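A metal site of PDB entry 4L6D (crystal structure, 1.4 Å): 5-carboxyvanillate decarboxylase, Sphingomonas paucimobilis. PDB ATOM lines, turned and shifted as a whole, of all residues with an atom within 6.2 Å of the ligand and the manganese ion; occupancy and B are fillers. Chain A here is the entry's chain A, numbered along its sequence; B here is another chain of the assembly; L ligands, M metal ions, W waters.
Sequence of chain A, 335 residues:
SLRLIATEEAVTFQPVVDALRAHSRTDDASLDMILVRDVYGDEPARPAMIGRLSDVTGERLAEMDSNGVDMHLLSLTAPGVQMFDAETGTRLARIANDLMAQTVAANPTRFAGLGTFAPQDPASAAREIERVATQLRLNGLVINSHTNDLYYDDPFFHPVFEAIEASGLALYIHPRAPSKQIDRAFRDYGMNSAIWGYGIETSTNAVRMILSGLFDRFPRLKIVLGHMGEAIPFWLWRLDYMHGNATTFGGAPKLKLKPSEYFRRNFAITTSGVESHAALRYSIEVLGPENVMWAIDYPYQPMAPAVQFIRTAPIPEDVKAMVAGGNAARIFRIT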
ATOM      1  N   GLU A   8     -11.559  -7.711 -11.395  1.00  0.00           N
ATOM      2  CA  GLU A   8     -11.021  -8.530 -12.488  1.00  0.00           C
ATOM      3  C   GLU A   8     -12.047  -8.677 -13.606  1.00  0.00           C
ATOM      4  O   GLU A   8     -12.428  -9.792 -13.979  1.00  0.00           O
ATOM      5  CB  GLU A   8     -10.571  -9.924 -12.022  1.00  0.00           C
ATOM      6  CG  GLU A   8      -9.542 -10.548 -12.990  1.00  0.00           C
ATOM      7  CD  GLU A   8      -9.228 -12.002 -12.671  1.00  0.00           C
ATOM      8  OE1 GLU A   8      -8.642 -12.264 -11.590  1.00  0.00           O
ATOM      9  OE2 GLU A   8      -9.556 -12.888 -13.492  1.00  0.00           O
ATOM     10  N   GLU A   9     -12.479  -7.543 -14.150  1.00  0.00           N
ATOM     11  CA  GLU A   9     -13.648  -7.530 -14.992  1.00  0.00           C
ATOM     12  C   GLU A   9     -13.218  -7.295 -16.418  1.00  0.00           C
ATOM     13  O   GLU A   9     -12.761  -6.216 -16.777  1.00  0.00           O
ATOM     14  CB  GLU A   9     -14.655  -6.485 -14.479  1.00  0.00           C
ATOM     15  CG  GLU A   9     -14.835  -6.574 -12.951  1.00  0.00           C
ATOM     16  CD  GLU A   9     -15.005  -8.009 -12.478  1.00  0.00           C
ATOM     17  OE1 GLU A   9     -14.338  -8.424 -11.491  1.00  0.00           O
ATOM     18  OE2 GLU A   9     -15.804  -8.739 -13.110  1.00  0.00           O
ATOM     19  N   ALA A  10     -13.350  -8.341 -17.225  1.00  0.00           N
ATOM     20  CA  ALA A  10     -12.809  -8.373 -18.575  1.00  0.00           C
ATOM     21  C   ALA A  10     -13.642  -7.571 -19.557  1.00  0.00           C
ATOM     22  O   ALA A  10     -14.878  -7.517 -19.458  1.00  0.00           O
ATOM     23  CB  ALA A  10     -12.710  -9.818 -19.047  1.00  0.00           C
ATOM     24  N   LEU A  35      -8.728 -21.281 -26.279  1.00  0.00           N
ATOM     25  CA  LEU A  35      -9.588 -20.138 -25.986  1.00  0.00           C
ATOM     26  C   LEU A  35      -9.824 -19.286 -27.235  1.00  0.00           C
ATOM     27  O   LEU A  35     -10.965 -18.907 -27.531  1.00  0.00           O
ATOM     28  CB  LEU A  35      -8.937 -19.252 -24.917  1.00  0.00           C
ATOM     29  CG  LEU A  35      -9.537 -17.857 -24.726  1.00  0.00           C
ATOM     30  CD1 LEU A  35     -10.879 -17.973 -24.047  1.00  0.00           C
ATOM     31  CD2 LEU A  35      -8.589 -16.978 -23.928  1.00  0.00           C
ATOM     32  N   ARG A  46     -18.048 -20.757 -28.400  1.00  0.00           N
ATOM     33  CA  ARG A  46     -18.584 -19.826 -27.394  1.00  0.00           C
ATOM     34  C   ARG A  46     -18.957 -18.520 -28.096  1.00  0.00           C
ATOM     35  O   ARG A  46     -18.315 -17.483 -27.887  1.00  0.00           O
ATOM     36  CB  ARG A  46     -17.553 -19.589 -26.274  1.00  0.00           C
ATOM     37  CG  ARG A  46     -17.134 -20.887 -25.550  1.00  0.00           C
ATOM     38  CD  ARG A  46     -15.919 -20.734 -24.611  1.00  0.00           C
ATOM     39  NE  ARG A  46     -16.264 -20.088 -23.334  1.00  0.00           N
ATOM     40  CZ  ARG A  46     -15.393 -19.831 -22.367  1.00  0.00           C
ATOM     41  NH1 ARG A  46     -14.113 -20.156 -22.514  1.00  0.00           N
ATOM     42  NH2 ARG A  46     -15.807 -19.258 -21.238  1.00  0.00           N
ATOM     43  N   MET A  49     -19.618 -14.805 -26.450  1.00  0.00           N
ATOM     44  CA  MET A  49     -18.629 -14.179 -25.583  1.00  0.00           C
ATOM     45  C   MET A  49     -18.075 -12.841 -26.094  1.00  0.00           C
ATOM     46  O   MET A  49     -17.873 -11.928 -25.297  1.00  0.00           O
ATOM     47  CB  MET A  49     -17.515 -15.159 -25.256  1.00  0.00           C
ATOM     48  CG  MET A  49     -16.573 -14.677 -24.168  1.00  0.00           C
ATOM     49  SD  MET A  49     -17.387 -14.358 -22.581  1.00  0.00           S
ATOM     50  CE  MET A  49     -17.544 -15.999 -21.898  1.00  0.00           C
ATOM     51  N   THR A  77      -9.208  -8.357 -21.888  1.00  0.00           N
ATOM     52  CA  THR A  77      -9.281  -9.774 -21.555  1.00  0.00           C
ATOM     53  C   THR A  77      -8.055 -10.528 -22.056  1.00  0.00           C
ATOM     54  O   THR A  77      -7.471 -10.160 -23.071  1.00  0.00           O
ATOM     55  CB  THR A  77     -10.576 -10.382 -22.146  1.00  0.00           C
ATOM     56  OG1 THR A  77     -10.758 -11.707 -21.638  1.00  0.00           O
ATOM     57  CG2 THR A  77     -10.557 -10.386 -23.672  1.00  0.00           C
ATOM     58  N   ALA A  78      -7.655 -11.556 -21.321  1.00  0.00           N
ATOM     59  CA  ALA A  78      -6.575 -12.425 -21.773  1.00  0.00           C
ATOM     60  C   ALA A  78      -6.959 -12.995 -23.148  1.00  0.00           C
ATOM     61  O   ALA A  78      -8.129 -13.276 -23.416  1.00  0.00           O
ATOM     62  CB  ALA A  78      -6.366 -13.550 -20.772  1.00  0.00           C
ATOM     63  N   PRO A  79      -5.963 -13.190 -24.034  1.00  0.00           N
ATOM     64  CA  PRO A  79      -4.513 -13.019 -23.851  1.00  0.00           C
ATOM     65  C   PRO A  79      -4.000 -11.614 -24.144  1.00  0.00           C
ATOM     66  O   PRO A  79      -2.808 -11.441 -24.425  1.00  0.00           O
ATOM     67  CB  PRO A  79      -3.940 -14.002 -24.868  1.00  0.00           C
ATOM     68  CG  PRO A  79      -4.916 -13.911 -26.012  1.00  0.00           C
ATOM     69  CD  PRO A  79      -6.278 -13.744 -25.365  1.00  0.00           C
ATOM     70  N   HIS A 174      -2.849 -11.243 -14.629  1.00  0.00           N
ATOM     71  CA  HIS A 174      -3.991 -12.106 -14.917  1.00  0.00           C
ATOM     72  C   HIS A 174      -3.473 -13.396 -15.546  1.00  0.00           C
ATOM     73  O   HIS A 174      -2.380 -13.402 -16.112  1.00  0.00           O
ATOM     74  CB  HIS A 174      -4.898 -11.350 -15.885  1.00  0.00           C
ATOM     75  CG  HIS A 174      -6.205 -12.015 -16.155  1.00  0.00           C
ATOM     76  ND1 HIS A 174      -6.352 -13.018 -17.099  1.00  0.00           N
ATOM     77  CD2 HIS A 174      -7.430 -11.833 -15.614  1.00  0.00           C
ATOM     78  CE1 HIS A 174      -7.611 -13.420 -17.122  1.00  0.00           C
ATOM     79  NE2 HIS A 174      -8.280 -12.721 -16.227  1.00  0.00           N
ATOM     80  N   PRO A 175      -4.237 -14.494 -15.468  1.00  0.00           N
ATOM     81  CA  PRO A 175      -3.751 -15.701 -16.166  1.00  0.00           C
ATOM     82  C   PRO A 175      -3.815 -15.632 -17.702  1.00  0.00           C
ATOM     83  O   PRO A 175      -4.453 -14.777 -18.321  1.00  0.00           O
ATOM     84  CB  PRO A 175      -4.716 -16.801 -15.676  1.00  0.00           C
ATOM     85  CG  PRO A 175      -5.272 -16.266 -14.384  1.00  0.00           C
ATOM     86  CD  PRO A 175      -5.362 -14.786 -14.560  1.00  0.00           C
ATOM     87  N   SER A 193      -7.468 -24.252 -19.176  1.00  0.00           N
ATOM     88  CA  SER A 193      -8.208 -23.055 -18.830  1.00  0.00           C
ATOM     89  C   SER A 193      -8.248 -22.819 -17.316  1.00  0.00           C
ATOM     90  O   SER A 193      -7.345 -23.239 -16.567  1.00  0.00           O
ATOM     91  CB  SER A 193      -9.629 -23.186 -19.434  1.00  0.00           C
ATOM     92  OG  SER A 193     -10.388 -21.993 -19.316  1.00  0.00           O
ATOM     93  N   ALA A 194      -9.309 -22.161 -16.860  1.00  0.00           N
ATOM     94  CA  ALA A 194      -9.456 -21.747 -15.473  1.00  0.00           C
ATOM     95  C   ALA A 194      -9.489 -22.891 -14.458  1.00  0.00           C
ATOM     96  O   ALA A 194      -9.096 -22.697 -13.299  1.00  0.00           O
ATOM     97  CB  ALA A 194     -10.699 -20.873 -15.330  1.00  0.00           C
ATOM     98  N   TYR A 198      -4.666 -22.239 -15.714  1.00  0.00           N
ATOM     99  CA  TYR A 198      -4.501 -20.812 -15.427  1.00  0.00           C
ATOM    100  C   TYR A 198      -3.753 -20.567 -14.113  1.00  0.00           C
ATOM    101  O   TYR A 198      -2.862 -19.718 -14.044  1.00  0.00           O
ATOM    102  CB  TYR A 198      -5.870 -20.110 -15.385  1.00  0.00           C
ATOM    103  CG  TYR A 198      -6.408 -19.722 -16.746  1.00  0.00           C
ATOM    104  CD1 TYR A 198      -5.825 -20.201 -17.925  1.00  0.00           C
ATOM    105  CD2 TYR A 198      -7.486 -18.850 -16.848  1.00  0.00           C
ATOM    106  CE1 TYR A 198      -6.329 -19.818 -19.180  1.00  0.00           C
ATOM    107  CE2 TYR A 198      -8.003 -18.476 -18.085  1.00  0.00           C
ATOM    108  CZ  TYR A 198      -7.411 -18.966 -19.247  1.00  0.00           C
ATOM    109  OH  TYR A 198      -7.909 -18.564 -20.470  1.00  0.00           O
ATOM    110  N   HIS A 227      -7.933 -14.989  -8.281  1.00  0.00           N
ATOM    111  CA  HIS A 227      -8.163 -16.399  -7.944  1.00  0.00           C
ATOM    112  C   HIS A 227      -7.513 -16.760  -6.630  1.00  0.00           C
ATOM    113  O   HIS A 227      -6.789 -17.757  -6.505  1.00  0.00           O
ATOM    114  CB  HIS A 227      -7.732 -17.271  -9.130  1.00  0.00           C
ATOM    115  CG  HIS A 227      -8.155 -16.660 -10.417  1.00  0.00           C
ATOM    116  ND1 HIS A 227      -7.262 -16.079 -11.289  1.00  0.00           N
ATOM    117  CD2 HIS A 227      -9.390 -16.392 -10.907  1.00  0.00           C
ATOM    118  CE1 HIS A 227      -7.926 -15.515 -12.281  1.00  0.00           C
ATOM    119  NE2 HIS A 227      -9.224 -15.691 -12.070  1.00  0.00           N
ATOM    120  N   SER A 272     -11.467 -13.320  -7.322  1.00  0.00           N
ATOM    121  CA  SER A 272     -12.089 -13.752  -8.576  1.00  0.00           C
ATOM    122  C   SER A 272     -12.128 -15.270  -8.685  1.00  0.00           C
ATOM    123  O   SER A 272     -11.114 -15.942  -8.482  1.00  0.00           O
ATOM    124  CB  SER A 272     -11.334 -13.187  -9.773  1.00  0.00           C
ATOM    125  OG  SER A 272      -9.947 -13.473  -9.658  1.00  0.00           O
ATOM    126  N   ASP A 297     -14.802 -11.625 -11.977  1.00  0.00           N
ATOM    127  CA  ASP A 297     -14.376 -12.296 -13.207  1.00  0.00           C
ATOM    128  C   ASP A 297     -15.503 -12.309 -14.266  1.00  0.00           C
ATOM    129  O   ASP A 297     -15.639 -13.266 -15.020  1.00  0.00           O
ATOM    130  CB  ASP A 297     -13.857 -13.717 -12.949  1.00  0.00           C
ATOM    131  CG  ASP A 297     -12.537 -13.991 -13.647  1.00  0.00           C
ATOM    132  OD1 ASP A 297     -12.209 -13.282 -14.612  1.00  0.00           O
ATOM    133  OD2 ASP A 297     -11.830 -14.925 -13.216  1.00  0.00           O
ATOM    134  N   TYR A 298     -16.293 -11.241 -14.307  1.00  0.00           N
ATOM    135  CA  TYR A 298     -17.311 -11.050 -15.345  1.00  0.00           C
ATOM    136  C   TYR A 298     -16.576 -10.761 -16.669  1.00  0.00           C
ATOM    137  O   TYR A 298     -15.544 -10.117 -16.662  1.00  0.00           O
ATOM    138  CB  TYR A 298     -18.208  -9.877 -14.952  1.00  0.00           C
ATOM    139  CG  TYR A 298     -19.315  -9.613 -15.928  1.00  0.00           C
ATOM    140  CD1 TYR A 298     -20.542 -10.261 -15.810  1.00  0.00           C
ATOM    141  CD2 TYR A 298     -19.139  -8.735 -16.997  1.00  0.00           C
ATOM    142  CE1 TYR A 298     -21.555 -10.033 -16.713  1.00  0.00           C
ATOM    143  CE2 TYR A 298     -20.152  -8.507 -17.900  1.00  0.00           C
ATOM    144  CZ  TYR A 298     -21.365  -9.156 -17.756  1.00  0.00           C
ATOM    145  OH  TYR A 298     -22.383  -8.948 -18.646  1.00  0.00           O
ATOM    146  N   TYR A 300     -16.995 -13.955 -17.586  1.00  0.00           N
ATOM    147  CA  TYR A 300     -16.731 -15.380 -17.510  1.00  0.00           C
ATOM    148  C   TYR A 300     -17.455 -16.046 -16.335  1.00  0.00           C
ATOM    149  O   TYR A 300     -17.671 -17.258 -16.347  1.00  0.00           O
ATOM    150  CB  TYR A 300     -15.223 -15.620 -17.469  1.00  0.00           C
ATOM    151  CG  TYR A 300     -14.510 -15.082 -18.701  1.00  0.00           C
ATOM    152  CD1 TYR A 300     -14.577 -15.761 -19.920  1.00  0.00           C
ATOM    153  CD2 TYR A 300     -13.780 -13.895 -18.656  1.00  0.00           C
ATOM    154  CE1 TYR A 300     -13.941 -15.272 -21.058  1.00  0.00           C
ATOM    155  CE2 TYR A 300     -13.130 -13.406 -19.790  1.00  0.00           C
ATOM    156  CZ  TYR A 300     -13.219 -14.095 -20.986  1.00  0.00           C
ATOM    157  OH  TYR A 300     -12.579 -13.616 -22.116  1.00  0.00           O
ATOM    158  N   GLN A 301     -17.803 -15.244 -15.332  1.00  0.00           N
ATOM    159  CA  GLN A 301     -18.644 -15.683 -14.219  1.00  0.00           C
ATOM    160  C   GLN A 301     -19.749 -14.666 -13.995  1.00  0.00           C
ATOM    161  O   GLN A 301     -19.592 -13.494 -14.350  1.00  0.00           O
ATOM    162  CB  GLN A 301     -17.822 -15.860 -12.953  1.00  0.00           C
ATOM    163  CG  GLN A 301     -16.781 -16.945 -13.101  1.00  0.00           C
ATOM    164  CD  GLN A 301     -16.325 -17.529 -11.774  1.00  0.00           C
ATOM    165  OE1 GLN A 301     -15.266 -18.109 -11.704  1.00  0.00           O
ATOM    166  NE2 GLN A 301     -17.156 -17.416 -10.742  1.00  0.00           N
ATOM    167  N   ARG B 238     -13.031 -23.649  -7.049  1.00  0.00           N
ATOM    168  CA  ARG B 238     -12.762 -23.338  -8.443  1.00  0.00           C
ATOM    169  C   ARG B 238     -12.780 -24.587  -9.319  1.00  0.00           C
ATOM    170  O   ARG B 238     -13.243 -24.559 -10.454  1.00  0.00           O
ATOM    171  CB  ARG B 238     -11.424 -22.605  -8.548  1.00  0.00           C
ATOM    172  CG  ARG B 238     -11.019 -22.149  -9.950  1.00  0.00           C
ATOM    173  CD  ARG B 238     -10.192 -20.889  -9.771  1.00  0.00           C
ATOM    174  NE  ARG B 238      -9.463 -20.403 -10.947  1.00  0.00           N
ATOM    175  CZ  ARG B 238      -9.978 -19.627 -11.883  1.00  0.00           C
ATOM    176  NH1 ARG B 238     -11.270 -19.299 -11.842  1.00  0.00           N
ATOM    177  NH2 ARG B 238      -9.211 -19.187 -12.877  1.00  0.00           N
ATOM    178  N   MET B 242     -15.545 -24.589 -12.365  1.00  0.00           N
ATOM    179  CA  MET B 242     -15.117 -24.635 -13.758  1.00  0.00           C
ATOM    180  C   MET B 242     -15.336 -25.981 -14.431  1.00  0.00           C
ATOM    181  O   MET B 242     -15.092 -26.124 -15.630  1.00  0.00           O
ATOM    182  CB  MET B 242     -13.649 -24.209 -13.855  1.00  0.00           C
ATOM    183  CG  MET B 242     -13.458 -22.699 -13.714  1.00  0.00           C
ATOM    184  SD  MET B 242     -14.378 -21.806 -14.974  1.00  0.00           S
ATOM    185  CE  MET B 242     -14.158 -20.087 -14.430  1.00  0.00           C
ATOM    186  N   ASN B 245     -17.488 -26.076 -17.680  1.00  0.00           N
ATOM    187  CA  ASN B 245     -16.788 -25.638 -18.888  1.00  0.00           C
ATOM    188  C   ASN B 245     -15.901 -26.757 -19.410  1.00  0.00           C
ATOM    189  O   ASN B 245     -15.753 -26.945 -20.617  1.00  0.00           O
ATOM    190  CB  ASN B 245     -15.938 -24.401 -18.621  1.00  0.00           C
ATOM    191  CG  ASN B 245     -16.765 -23.136 -18.486  1.00  0.00           C
ATOM    192  OD1 ASN B 245     -17.932 -23.083 -18.898  1.00  0.00           O
ATOM    193  ND2 ASN B 245     -16.150 -22.095 -17.923  1.00  0.00           N
HETATM  194  C1  LIG L   1     -12.157 -17.701 -18.755  1.00  0.00           C
HETATM  195  C2  LIG L   1     -12.385 -17.372 -17.408  1.00  0.00           C
HETATM  196  C3  LIG L   1     -11.338 -16.898 -19.567  1.00  0.00           C
HETATM  197  C4  LIG L   1     -11.806 -16.220 -16.855  1.00  0.00           C
HETATM  198  C5  LIG L   1     -10.746 -15.756 -19.032  1.00  0.00           C
HETATM  199  O1  LIG L   1      -9.937 -14.914 -19.758  1.00  0.00           O
HETATM  200  C6  LIG L   1     -10.989 -15.398 -17.631  1.00  0.00           C
HETATM  201  C7  LIG L   1     -12.820 -18.919 -19.334  1.00  0.00           C
HETATM  202  C8  LIG L   1      -9.631 -15.195 -21.132  1.00  0.00           C
HETATM  203  O2  LIG L   1     -13.777 -19.480 -18.733  1.00  0.00           O
HETATM  204  O3  LIG L   1     -12.448 -19.319 -20.467  1.00  0.00           O
HETATM  205  O4  LIG L   1     -10.660 -14.119 -17.279  1.00  0.00           O
HETATM  206 MN    MN M   1     -10.320 -13.136 -15.522  1.00  0.00          MN
HETATM  207  O   HOH W   1     -16.317 -19.250 -17.688  1.00  0.00           O
HETATM  208  O   HOH W   2      -9.748 -12.134 -19.124  1.00  0.00           O
HETATM  209  O   HOH W   3     -10.048 -20.124 -21.080  1.00  0.00           O
HETATM  210  O   HOH W   4     -11.005 -11.128 -16.105  1.00  0.00           O
HETATM  211  O   HOH W   5     -10.011 -17.135 -14.688  1.00  0.00           O
HETATM  212  O   HOH W   6     -13.236 -22.120 -19.088  1.00  0.00           O
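Water W3 lies within hydrogen-bond range of OG of Ser 193 (2.6 Å), O3 of the ligand (2.6 Å) and OH of Tyr 198 (2.7 Å).
Water W6 lies within hydrogen-bond range of an oxygen (O2) of the ligand (2.7 Å), the side-chain hydroxyl (OG) of Ser 193 (2.9 Å) and the side-chain amide nitrogen (ND2) of Asn 245 of chain B (3.1 Å).
Water W1 lies within hydrogen-bond range of the backbone carbonyl oxygen (O) of Tyr 300 (2.8 Å), an oxygen (O2) of the ligand (2.8 Å) and the side-chain amide nitrogen (ND2) of Asn 245 of chain B (2.9 Å).
Water W2 lies within hydrogen-bond range of OG1 of Thr 77 (2.7 Å), O1 of the ligand (2.9 Å) and N of Ala 78 (3.1 Å).
Water W5 lies within hydrogen-bond range of the guanidinium group of Arg 238 of chain B, a ring nitrogen (NE2) of His 227 and the side-chain carboxylate of Asp 297.
The manganese ion is bound by an oxygen (O4) of the ligand (2.0 Å), the side-chain carboxylate (OD1) of Asp 297 (2.1 Å), the side-chain carboxylate (OE2) of Glu 8 (2.2 Å), a ring nitrogen (NE2) of His 174 (2.2 Å) and water W4 (2.2 Å).
Of the 23 residues printed, 3 come within 4 Å of the manganese ion.
The nearest printed residue that does not touch the manganese ion is His 227 (4.4 Å).
Merely in contact with the ligand: Leu 35, Thr 77, Ala 78, Ser 193, Tyr 198, Tyr 300 and Asn 245 of chain B.
Hydrophobic or aromatic side chains that line the ligand: Leu 35, Ala 78, His 174, Tyr 198 and Tyr 300.
Of the 23 residues printed, 10 come within 4 Å of the ligand.
The nearest printed residue that does not touch the ligand is Glu 8 (4.1 Å).
NH1 of Arg 46 is in salt-bridge range of O3 of the ligand (2.8 Å).
A ring nitrogen (NE2) of His 227 is in hydrogen-bond range of the side-chain carboxylate (OD2) of Asp 297, at 2.9 Å.
N of Asp 297 is in hydrogen-bond range of OE2 of Glu 9 (3.3 Å).
OE2 of Glu 8 lies close to NE2 of His 227 (3.2 Å).
The side-chain hydroxyl (OG) of Ser 272 lies within hydrogen-bond range of the side-chain carboxylate (OE1) of Glu 8, 2.6 Å away.
The side-chain hydroxyl (OH) of Tyr 300 lies within hydrogen-bond range of the side-chain hydroxyl (OG1) of Thr 77 (2.7 Å).
The backbone NH of Tyr 198 sits at hydrogen-bond distance from the backbone carbonyl oxygen of Ser 193 (3.0 Å).
The side-chain amide nitrogen (ND2) of Asn 245 of chain B lies within hydrogen-bond range of the side-chain sulfur (SD) of Met 242 of chain B (3.5 Å).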
